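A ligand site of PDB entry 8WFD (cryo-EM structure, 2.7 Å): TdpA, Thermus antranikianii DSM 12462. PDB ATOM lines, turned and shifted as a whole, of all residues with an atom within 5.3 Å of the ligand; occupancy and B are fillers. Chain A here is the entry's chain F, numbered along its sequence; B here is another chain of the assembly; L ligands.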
ATOM      1  N   LYS A 194      34.276  23.038 -19.914  1.00  0.00           N
ATOM      2  CA  LYS A 194      33.505  22.218 -18.991  1.00  0.00           C
ATOM      3  C   LYS A 194      32.015  22.329 -19.319  1.00  0.00           C
ATOM      4  O   LYS A 194      31.581  23.191 -20.089  1.00  0.00           O
ATOM      5  CB  LYS A 194      33.778  22.644 -17.558  1.00  0.00           C
ATOM      6  CG  LYS A 194      33.432  21.594 -16.526  1.00  0.00           C
ATOM      7  CD  LYS A 194      34.073  21.917 -15.201  1.00  0.00           C
ATOM      8  CE  LYS A 194      33.314  21.262 -14.059  1.00  0.00           C
ATOM      9  NZ  LYS A 194      34.126  21.179 -12.814  1.00  0.00           N
ATOM     10  N   THR A 195      31.231  21.439 -18.732  1.00  0.00           N
ATOM     11  CA  THR A 195      29.796  21.398 -19.001  1.00  0.00           C
ATOM     12  C   THR A 195      29.108  22.549 -18.279  1.00  0.00           C
ATOM     13  O   THR A 195      29.197  22.667 -17.051  1.00  0.00           O
ATOM     14  CB  THR A 195      29.208  20.057 -18.555  1.00  0.00           C
ATOM     15  OG1 THR A 195      27.803  20.058 -18.830  1.00  0.00           O
ATOM     16  CG2 THR A 195      29.387  19.887 -17.071  1.00  0.00           C
ATOM     17  N   GLY A 196      28.408  23.391 -19.038  1.00  0.00           N
ATOM     18  CA  GLY A 196      27.674  24.500 -18.502  1.00  0.00           C
ATOM     19  C   GLY A 196      28.340  25.842 -18.628  1.00  0.00           C
ATOM     20  O   GLY A 196      27.907  26.797 -17.972  1.00  0.00           O
ATOM     21  N   PHE A 197      29.384  25.961 -19.456  1.00  0.00           N
ATOM     22  CA  PHE A 197      30.188  27.168 -19.511  1.00  0.00           C
ATOM     23  C   PHE A 197      30.074  27.931 -20.820  1.00  0.00           C
ATOM     24  O   PHE A 197      30.666  29.000 -20.945  1.00  0.00           O
ATOM     25  CB  PHE A 197      31.660  26.832 -19.221  1.00  0.00           C
ATOM     26  CG  PHE A 197      31.947  26.636 -17.758  1.00  0.00           C
ATOM     27  CD1 PHE A 197      31.617  25.453 -17.124  1.00  0.00           C
ATOM     28  CD2 PHE A 197      32.513  27.651 -17.007  1.00  0.00           C
ATOM     29  CE1 PHE A 197      31.858  25.283 -15.781  1.00  0.00           C
ATOM     30  CE2 PHE A 197      32.769  27.483 -15.662  1.00  0.00           C
ATOM     31  CZ  PHE A 197      32.441  26.296 -15.045  1.00  0.00           C
ATOM     32  N   GLY A 198      29.324  27.420 -21.796  1.00  0.00           N
ATOM     33  CA  GLY A 198      28.950  28.244 -22.940  1.00  0.00           C
ATOM     34  C   GLY A 198      29.305  27.765 -24.329  1.00  0.00           C
ATOM     35  O   GLY A 198      29.291  28.560 -25.267  1.00  0.00           O
ATOM     36  N   LYS A 199      29.594  26.468 -24.502  1.00  0.00           N
ATOM     37  CA  LYS A 199      29.951  25.962 -25.822  1.00  0.00           C
ATOM     38  C   LYS A 199      28.797  26.122 -26.801  1.00  0.00           C
ATOM     39  O   LYS A 199      28.976  26.632 -27.915  1.00  0.00           O
ATOM     40  CB  LYS A 199      30.357  24.494 -25.723  1.00  0.00           C
ATOM     41  CG  LYS A 199      31.602  24.234 -24.900  1.00  0.00           C
ATOM     42  CD  LYS A 199      32.044  22.795 -25.047  1.00  0.00           C
ATOM     43  CE  LYS A 199      31.064  21.831 -24.416  1.00  0.00           C
ATOM     44  NZ  LYS A 199      30.943  22.005 -22.951  1.00  0.00           N
ATOM     45  N   SER A 200      27.594  25.691 -26.410  1.00  0.00           N
ATOM     46  CA  SER A 200      26.447  25.755 -27.312  1.00  0.00           C
ATOM     47  C   SER A 200      26.028  27.193 -27.587  1.00  0.00           C
ATOM     48  O   SER A 200      25.649  27.517 -28.720  1.00  0.00           O
ATOM     49  CB  SER A 200      25.287  24.948 -26.735  1.00  0.00           C
ATOM     50  OG  SER A 200      25.720  23.697 -26.235  1.00  0.00           O
ATOM     51  N   ASN A 201      26.091  28.062 -26.581  1.00  0.00           N
ATOM     52  CA  ASN A 201      25.786  29.472 -26.803  1.00  0.00           C
ATOM     53  C   ASN A 201      26.782  30.095 -27.780  1.00  0.00           C
ATOM     54  O   ASN A 201      26.393  30.870 -28.657  1.00  0.00           O
ATOM     55  CB  ASN A 201      25.783  30.221 -25.483  1.00  0.00           C
ATOM     56  CG  ASN A 201      25.373  31.667 -25.625  1.00  0.00           C
ATOM     57  OD1 ASN A 201      25.151  32.148 -26.735  1.00  0.00           O
ATOM     58  ND2 ASN A 201      25.278  32.372 -24.517  1.00  0.00           N
ATOM     59  N   GLU A 227      18.132  20.647 -29.270  1.00  0.00           N
ATOM     60  CA  GLU A 227      18.261  21.988 -28.719  1.00  0.00           C
ATOM     61  C   GLU A 227      18.505  23.072 -29.750  1.00  0.00           C
ATOM     62  O   GLU A 227      18.421  24.258 -29.397  1.00  0.00           O
ATOM     63  CB  GLU A 227      19.389  22.038 -27.676  1.00  0.00           C
ATOM     64  CG  GLU A 227      20.736  21.651 -28.243  1.00  0.00           C
ATOM     65  CD  GLU A 227      21.872  21.930 -27.287  1.00  0.00           C
ATOM     66  OE1 GLU A 227      21.629  22.587 -26.255  1.00  0.00           O
ATOM     67  OE2 GLU A 227      23.005  21.496 -27.558  1.00  0.00           O
ATOM     68  N   ALA A 234      14.944  27.022 -19.211  1.00  0.00           N
ATOM     69  CA  ALA A 234      15.954  27.956 -18.730  1.00  0.00           C
ATOM     70  C   ALA A 234      17.234  27.217 -18.364  1.00  0.00           C
ATOM     71  O   ALA A 234      17.763  27.370 -17.263  1.00  0.00           O
ATOM     72  CB  ALA A 234      15.434  28.731 -17.528  1.00  0.00           C
ATOM     73  N   THR A 235      17.751  26.426 -19.311  1.00  0.00           N
ATOM     74  CA  THR A 235      18.995  25.705 -19.121  1.00  0.00           C
ATOM     75  C   THR A 235      19.928  25.843 -20.317  1.00  0.00           C
ATOM     76  O   THR A 235      21.006  25.222 -20.315  1.00  0.00           O
ATOM     77  CB  THR A 235      18.727  24.214 -18.847  1.00  0.00           C
ATOM     78  OG1 THR A 235      19.888  23.592 -18.298  1.00  0.00           O
ATOM     79  CG2 THR A 235      18.334  23.501 -20.137  1.00  0.00           C
ATOM     80  N   THR A 236      19.564  26.622 -21.318  1.00  0.00           N
ATOM     81  CA  THR A 236      20.396  26.893 -22.484  1.00  0.00           C
ATOM     82  C   THR A 236      19.830  28.139 -23.167  1.00  0.00           C
ATOM     83  O   THR A 236      18.819  28.695 -22.736  1.00  0.00           O
ATOM     84  CB  THR A 236      20.429  25.681 -23.419  1.00  0.00           C
ATOM     85  OG1 THR A 236      20.873  24.523 -22.705  1.00  0.00           O
ATOM     86  CG2 THR A 236      21.385  25.910 -24.580  1.00  0.00           C
ATOM     87  N   SER A 237      20.502  28.575 -24.227  1.00  0.00           N
ATOM     88  CA  SER A 237      20.042  29.703 -25.003  1.00  0.00           C
ATOM     89  C   SER A 237      18.932  29.282 -25.957  1.00  0.00           C
ATOM     90  O   SER A 237      18.794  28.106 -26.288  1.00  0.00           O
ATOM     91  CB  SER A 237      21.199  30.324 -25.779  1.00  0.00           C
ATOM     92  OG  SER A 237      22.051  31.041 -24.921  1.00  0.00           O
ATOM     93  N   GLU A 473      28.407  18.266 -32.394  1.00  0.00           N
ATOM     94  CA  GLU A 473      28.509  18.300 -30.939  1.00  0.00           C
ATOM     95  C   GLU A 473      28.875  16.918 -30.415  1.00  0.00           C
ATOM     96  O   GLU A 473      28.495  15.894 -30.981  1.00  0.00           O
ATOM     97  CB  GLU A 473      27.208  18.781 -30.310  1.00  0.00           C
ATOM     98  CG  GLU A 473      26.875  20.236 -30.598  1.00  0.00           C
ATOM     99  CD  GLU A 473      27.079  21.147 -29.406  1.00  0.00           C
ATOM    100  OE1 GLU A 473      27.848  20.765 -28.500  1.00  0.00           O
ATOM    101  OE2 GLU A 473      26.478  22.232 -29.374  1.00  0.00           O
ATOM    102  N   GLN A 505      33.990  19.049 -25.010  1.00  0.00           N
ATOM    103  CA  GLN A 505      34.121  19.165 -23.554  1.00  0.00           C
ATOM    104  C   GLN A 505      35.485  18.758 -23.027  1.00  0.00           C
ATOM    105  O   GLN A 505      35.791  19.001 -21.853  1.00  0.00           O
ATOM    106  CB  GLN A 505      33.079  18.309 -22.825  1.00  0.00           C
ATOM    107  CG  GLN A 505      31.741  18.945 -22.545  1.00  0.00           C
ATOM    108  CD  GLN A 505      30.859  18.044 -21.712  1.00  0.00           C
ATOM    109  OE1 GLN A 505      31.250  16.938 -21.352  1.00  0.00           O
ATOM    110  NE2 GLN A 505      29.661  18.516 -21.384  1.00  0.00           N
ATOM    111  N   ILE A 555      31.895  31.582 -16.355  1.00  0.00           N
ATOM    112  CA  ILE A 555      30.987  31.102 -17.382  1.00  0.00           C
ATOM    113  C   ILE A 555      30.921  32.131 -18.505  1.00  0.00           C
ATOM    114  O   ILE A 555      30.623  33.305 -18.263  1.00  0.00           O
ATOM    115  CB  ILE A 555      29.595  30.816 -16.812  1.00  0.00           C
ATOM    116  CG1 ILE A 555      29.631  29.574 -15.921  1.00  0.00           C
ATOM    117  CG2 ILE A 555      28.576  30.654 -17.919  1.00  0.00           C
ATOM    118  CD1 ILE A 555      28.406  29.418 -15.057  1.00  0.00           C
ATOM    119  N   GLY A 556      31.186  31.698 -19.730  1.00  0.00           N
ATOM    120  CA  GLY A 556      31.144  32.580 -20.881  1.00  0.00           C
ATOM    121  C   GLY A 556      32.424  33.309 -21.175  1.00  0.00           C
ATOM    122  O   GLY A 556      32.407  34.279 -21.950  1.00  0.00           O
ATOM    123  N   ARG A 573      35.221  38.006 -23.730  1.00  0.00           N
ATOM    124  CA  ARG A 573      33.940  37.860 -23.050  1.00  0.00           C
ATOM    125  C   ARG A 573      32.922  37.663 -24.171  1.00  0.00           C
ATOM    126  O   ARG A 573      32.802  38.496 -25.067  1.00  0.00           O
ATOM    127  CB  ARG A 573      33.634  39.090 -22.203  1.00  0.00           C
ATOM    128  CG  ARG A 573      32.328  39.024 -21.447  1.00  0.00           C
ATOM    129  CD  ARG A 573      32.377  37.941 -20.390  1.00  0.00           C
ATOM    130  NE  ARG A 573      31.136  37.847 -19.644  1.00  0.00           N
ATOM    131  CZ  ARG A 573      30.847  36.869 -18.798  1.00  0.00           C
ATOM    132  NH1 ARG A 573      31.702  35.890 -18.555  1.00  0.00           N
ATOM    133  NH2 ARG A 573      29.669  36.873 -18.165  1.00  0.00           N
ATOM    134  N   VAL A 574      32.216  36.523 -24.127  1.00  0.00           N
ATOM    135  CA  VAL A 574      31.304  36.145 -25.201  1.00  0.00           C
ATOM    136  C   VAL A 574      29.905  36.669 -24.909  1.00  0.00           C
ATOM    137  O   VAL A 574      29.511  36.869 -23.754  1.00  0.00           O
ATOM    138  CB  VAL A 574      31.302  34.623 -25.385  1.00  0.00           C
ATOM    139  CG1 VAL A 574      30.548  34.235 -26.646  1.00  0.00           C
ATOM    140  CG2 VAL A 574      32.715  34.086 -25.446  1.00  0.00           C
ATOM    141  N   LYS A 575      29.140  36.876 -25.979  1.00  0.00           N
ATOM    142  CA  LYS A 575      27.825  37.495 -25.891  1.00  0.00           C
ATOM    143  C   LYS A 575      26.738  36.449 -25.733  1.00  0.00           C
ATOM    144  O   LYS A 575      26.792  35.368 -26.322  1.00  0.00           O
ATOM    145  CB  LYS A 575      27.563  38.340 -27.135  1.00  0.00           C
ATOM    146  CG  LYS A 575      28.408  39.584 -27.224  1.00  0.00           C
ATOM    147  CD  LYS A 575      28.174  40.319 -28.530  1.00  0.00           C
ATOM    148  CE  LYS A 575      28.753  41.725 -28.477  1.00  0.00           C
ATOM    149  NZ  LYS A 575      30.219  41.707 -28.204  1.00  0.00           N
ATOM    150  N   LEU A 576      25.730  36.784 -24.929  1.00  0.00           N
ATOM    151  CA  LEU A 576      24.533  35.956 -24.840  1.00  0.00           C
ATOM    152  C   LEU A 576      23.700  36.088 -26.110  1.00  0.00           C
ATOM    153  O   LEU A 576      23.605  37.177 -26.689  1.00  0.00           O
ATOM    154  CB  LEU A 576      23.703  36.348 -23.621  1.00  0.00           C
ATOM    155  CG  LEU A 576      23.867  35.536 -22.338  1.00  0.00           C
ATOM    156  CD1 LEU A 576      22.855  35.996 -21.307  1.00  0.00           C
ATOM    157  CD2 LEU A 576      23.715  34.060 -22.601  1.00  0.00           C
ATOM    158  N   LYS B 491      27.679  13.222 -18.745  1.00  0.00           N
ATOM    159  CA  LYS B 491      28.108  14.298 -19.629  1.00  0.00           C
ATOM    160  C   LYS B 491      26.956  15.000 -20.344  1.00  0.00           C
ATOM    161  O   LYS B 491      27.194  16.003 -21.018  1.00  0.00           O
ATOM    162  CB  LYS B 491      29.102  13.776 -20.658  1.00  0.00           C
ATOM    163  CG  LYS B 491      30.466  13.444 -20.072  1.00  0.00           C
ATOM    164  CD  LYS B 491      31.186  12.385 -20.888  1.00  0.00           C
ATOM    165  CE  LYS B 491      31.815  12.991 -22.120  1.00  0.00           C
ATOM    166  NZ  LYS B 491      32.957  13.873 -21.783  1.00  0.00           N
ATOM    167  N   ARG B 494      22.881  17.414 -17.550  1.00  0.00           N
ATOM    168  CA  ARG B 494      22.676  18.764 -17.016  1.00  0.00           C
ATOM    169  C   ARG B 494      21.544  19.475 -17.725  1.00  0.00           C
ATOM    170  O   ARG B 494      20.794  20.242 -17.101  1.00  0.00           O
ATOM    171  CB  ARG B 494      23.968  19.570 -17.135  1.00  0.00           C
ATOM    172  CG  ARG B 494      23.881  20.983 -16.590  1.00  0.00           C
ATOM    173  CD  ARG B 494      24.962  21.869 -17.168  1.00  0.00           C
ATOM    174  NE  ARG B 494      24.798  22.076 -18.599  1.00  0.00           N
ATOM    175  CZ  ARG B 494      23.983  22.980 -19.130  1.00  0.00           C
ATOM    176  NH1 ARG B 494      23.258  23.794 -18.381  1.00  0.00           N
ATOM    177  NH2 ARG B 494      23.885  23.065 -20.452  1.00  0.00           N
ATOM    178  N   LYS B 495      21.392  19.243 -19.030  1.00  0.00           N
ATOM    179  CA  LYS B 495      20.352  19.927 -19.798  1.00  0.00           C
ATOM    180  C   LYS B 495      18.952  19.555 -19.322  1.00  0.00           C
ATOM    181  O   LYS B 495      18.049  20.396 -19.303  1.00  0.00           O
ATOM    182  CB  LYS B 495      20.507  19.619 -21.280  1.00  0.00           C
ATOM    183  CG  LYS B 495      21.501  20.495 -22.006  1.00  0.00           C
ATOM    184  CD  LYS B 495      21.532  20.153 -23.489  1.00  0.00           C
ATOM    185  CE  LYS B 495      22.346  18.905 -23.740  1.00  0.00           C
ATOM    186  NZ  LYS B 495      23.791  19.108 -23.496  1.00  0.00           N
HETATM  187  P1  LIG L   1      26.884  21.475 -22.080  1.00  0.00           P
HETATM  188  O1  LIG L   1      25.908  20.676 -21.280  1.00  0.00           O
HETATM  189  O2  LIG L   1      28.282  20.772 -22.030  1.00  0.00           O
HETATM  190  O3  LIG L   1      26.399  21.583 -23.574  1.00  0.00           O
HETATM  191  P2  LIG L   1      27.372  24.180 -22.555  1.00  0.00           P
HETATM  192  O4  LIG L   1      26.732  23.839 -23.856  1.00  0.00           O
HETATM  193  O5  LIG L   1      28.905  24.229 -22.738  1.00  0.00           O
HETATM  194  N1  LIG L   1      26.999  23.026 -21.400  1.00  0.00           N
HETATM  195  P3  LIG L   1      25.465  26.137 -22.516  1.00  0.00           P
HETATM  196  O6  LIG L   1      24.439  25.086 -22.528  1.00  0.00           O
HETATM  197  O7  LIG L   1      25.672  26.804 -23.876  1.00  0.00           O
HETATM  198  O8  LIG L   1      26.876  25.577 -22.071  1.00  0.00           O
HETATM  199  O9  LIG L   1      25.081  27.212 -21.434  1.00  0.00           O
HETATM  200  C1  LIG L   1      24.435  26.856 -20.195  1.00  0.00           C
HETATM  201  C2  LIG L   1      24.121  28.111 -19.430  1.00  0.00           C
HETATM  202  O10 LIG L   1      25.318  28.886 -19.242  1.00  0.00           O
HETATM  203  C3  LIG L   1      23.148  29.067 -20.098  1.00  0.00           C
HETATM  204  O11 LIG L   1      21.791  28.707 -19.830  1.00  0.00           O
HETATM  205  C4  LIG L   1      23.506  30.407 -19.472  1.00  0.00           C
HETATM  206  O12 LIG L   1      22.816  30.619 -18.243  1.00  0.00           O
HETATM  207  C5  LIG L   1      25.012  30.274 -19.226  1.00  0.00           C
HETATM  208  N2  LIG L   1      25.838  30.931 -20.227  1.00  0.00           N
HETATM  209  C6  LIG L   1      26.407  30.373 -21.334  1.00  0.00           C
HETATM  210  N3  LIG L   1      27.097  31.217 -22.072  1.00  0.00           N
HETATM  211  C7  LIG L   1      26.971  32.416 -21.389  1.00  0.00           C
HETATM  212  C8  LIG L   1      27.477  33.704 -21.647  1.00  0.00           C
HETATM  213  N4  LIG L   1      28.238  34.004 -22.701  1.00  0.00           N
HETATM  214  N5  LIG L   1      27.168  34.685 -20.768  1.00  0.00           N
HETATM  215  C9  LIG L   1      26.412  34.392 -19.708  1.00  0.00           C
HETATM  216  N6  LIG L   1      25.875  33.212 -19.365  1.00  0.00           N
HETATM  217  C10 LIG L   1      26.195  32.257 -20.250  1.00  0.00           C
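N of Gly 196 sits close to N1 of the ligand, 2.8 Å away. Lys 194 touches the ligand. Phe 197 touches the ligand (N to O8, 3.6 Å). Thr 235 touches the ligand. CG2 of Ile 555 touches N2 of the ligand, 3.6 Å away. Gly 556 touches the ligand (CA to N4, 3.7 Å). Leu 576 touches the ligand. The nearest printed residue that does not touch the ligand is Lys 575 (4.1 Å).
The backbone NH (N) of Ser 200 is in hydrogen-bond range of an oxygen (O4) of the ligand (3.3 Å). The side-chain hydroxyl (OG) of Ser 200 sits at hydrogen-bond distance from an oxygen (O4) of the ligand. The side-chain amide nitrogen (NE2) of Gln 505 lies within hydrogen-bond range of an oxygen (O2) of the ligand. An oxygen (O5) of the ligand lies within hydrogen-bond range of the backbone NH (N) of Lys 199 (2.9 Å). An oxygen (O5) of the ligand lies within salt-bridge range of the side-chain amino group of Lys 199 (3.0 Å). An oxygen (O6) of the ligand lies within salt-bridge range of the guanidinium group of Arg 494 of chain B (2.9 Å). N of Asn 201 sits at hydrogen-bond distance from O7 of the ligand (3.0 Å). The side-chain amide nitrogen of Asn 201 sits at hydrogen-bond distance from a nitrogen (N3) of the ligand, 3.3 Å away. N of Gly 198 is in hydrogen-bond range of O8 of the ligand. An oxygen (O1) of the ligand lies within hydrogen-bond range of the side-chain hydroxyl (OG1) of Thr 195 (3.2 Å). The backbone carbonyl oxygen of Val 574 is in hydrogen-bond range of a nitrogen (N4) of the ligand (3.3 Å). An oxygen (O11) of the ligand lies within hydrogen-bond range of the backbone NH of Thr 236, 3.4 Å away. The side-chain amino group of Lys 495 of chain B lies within salt-bridge range of an oxygen (O1) of the ligand, at 3.4 Å.
The backbone carbonyl oxygen (O) of Lys 194 sits at hydrogen-bond distance from the side-chain amino group (NZ) of Lys 199, 3.2 Å away. NH1 of Arg 494 of chain B sits at hydrogen-bond distance from O of Thr 235 (3.3 Å). N of Val 574 sits at hydrogen-bond distance from O of Gly 556 (3.1 Å). The backbone carbonyl oxygen (O) of Ile 555 sits at hydrogen-bond distance from the guanidinium group (NH1) of Arg 573 (2.8 Å). N of Gly 556 lies within hydrogen-bond range of O of Phe 197, 3.0 Å away.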
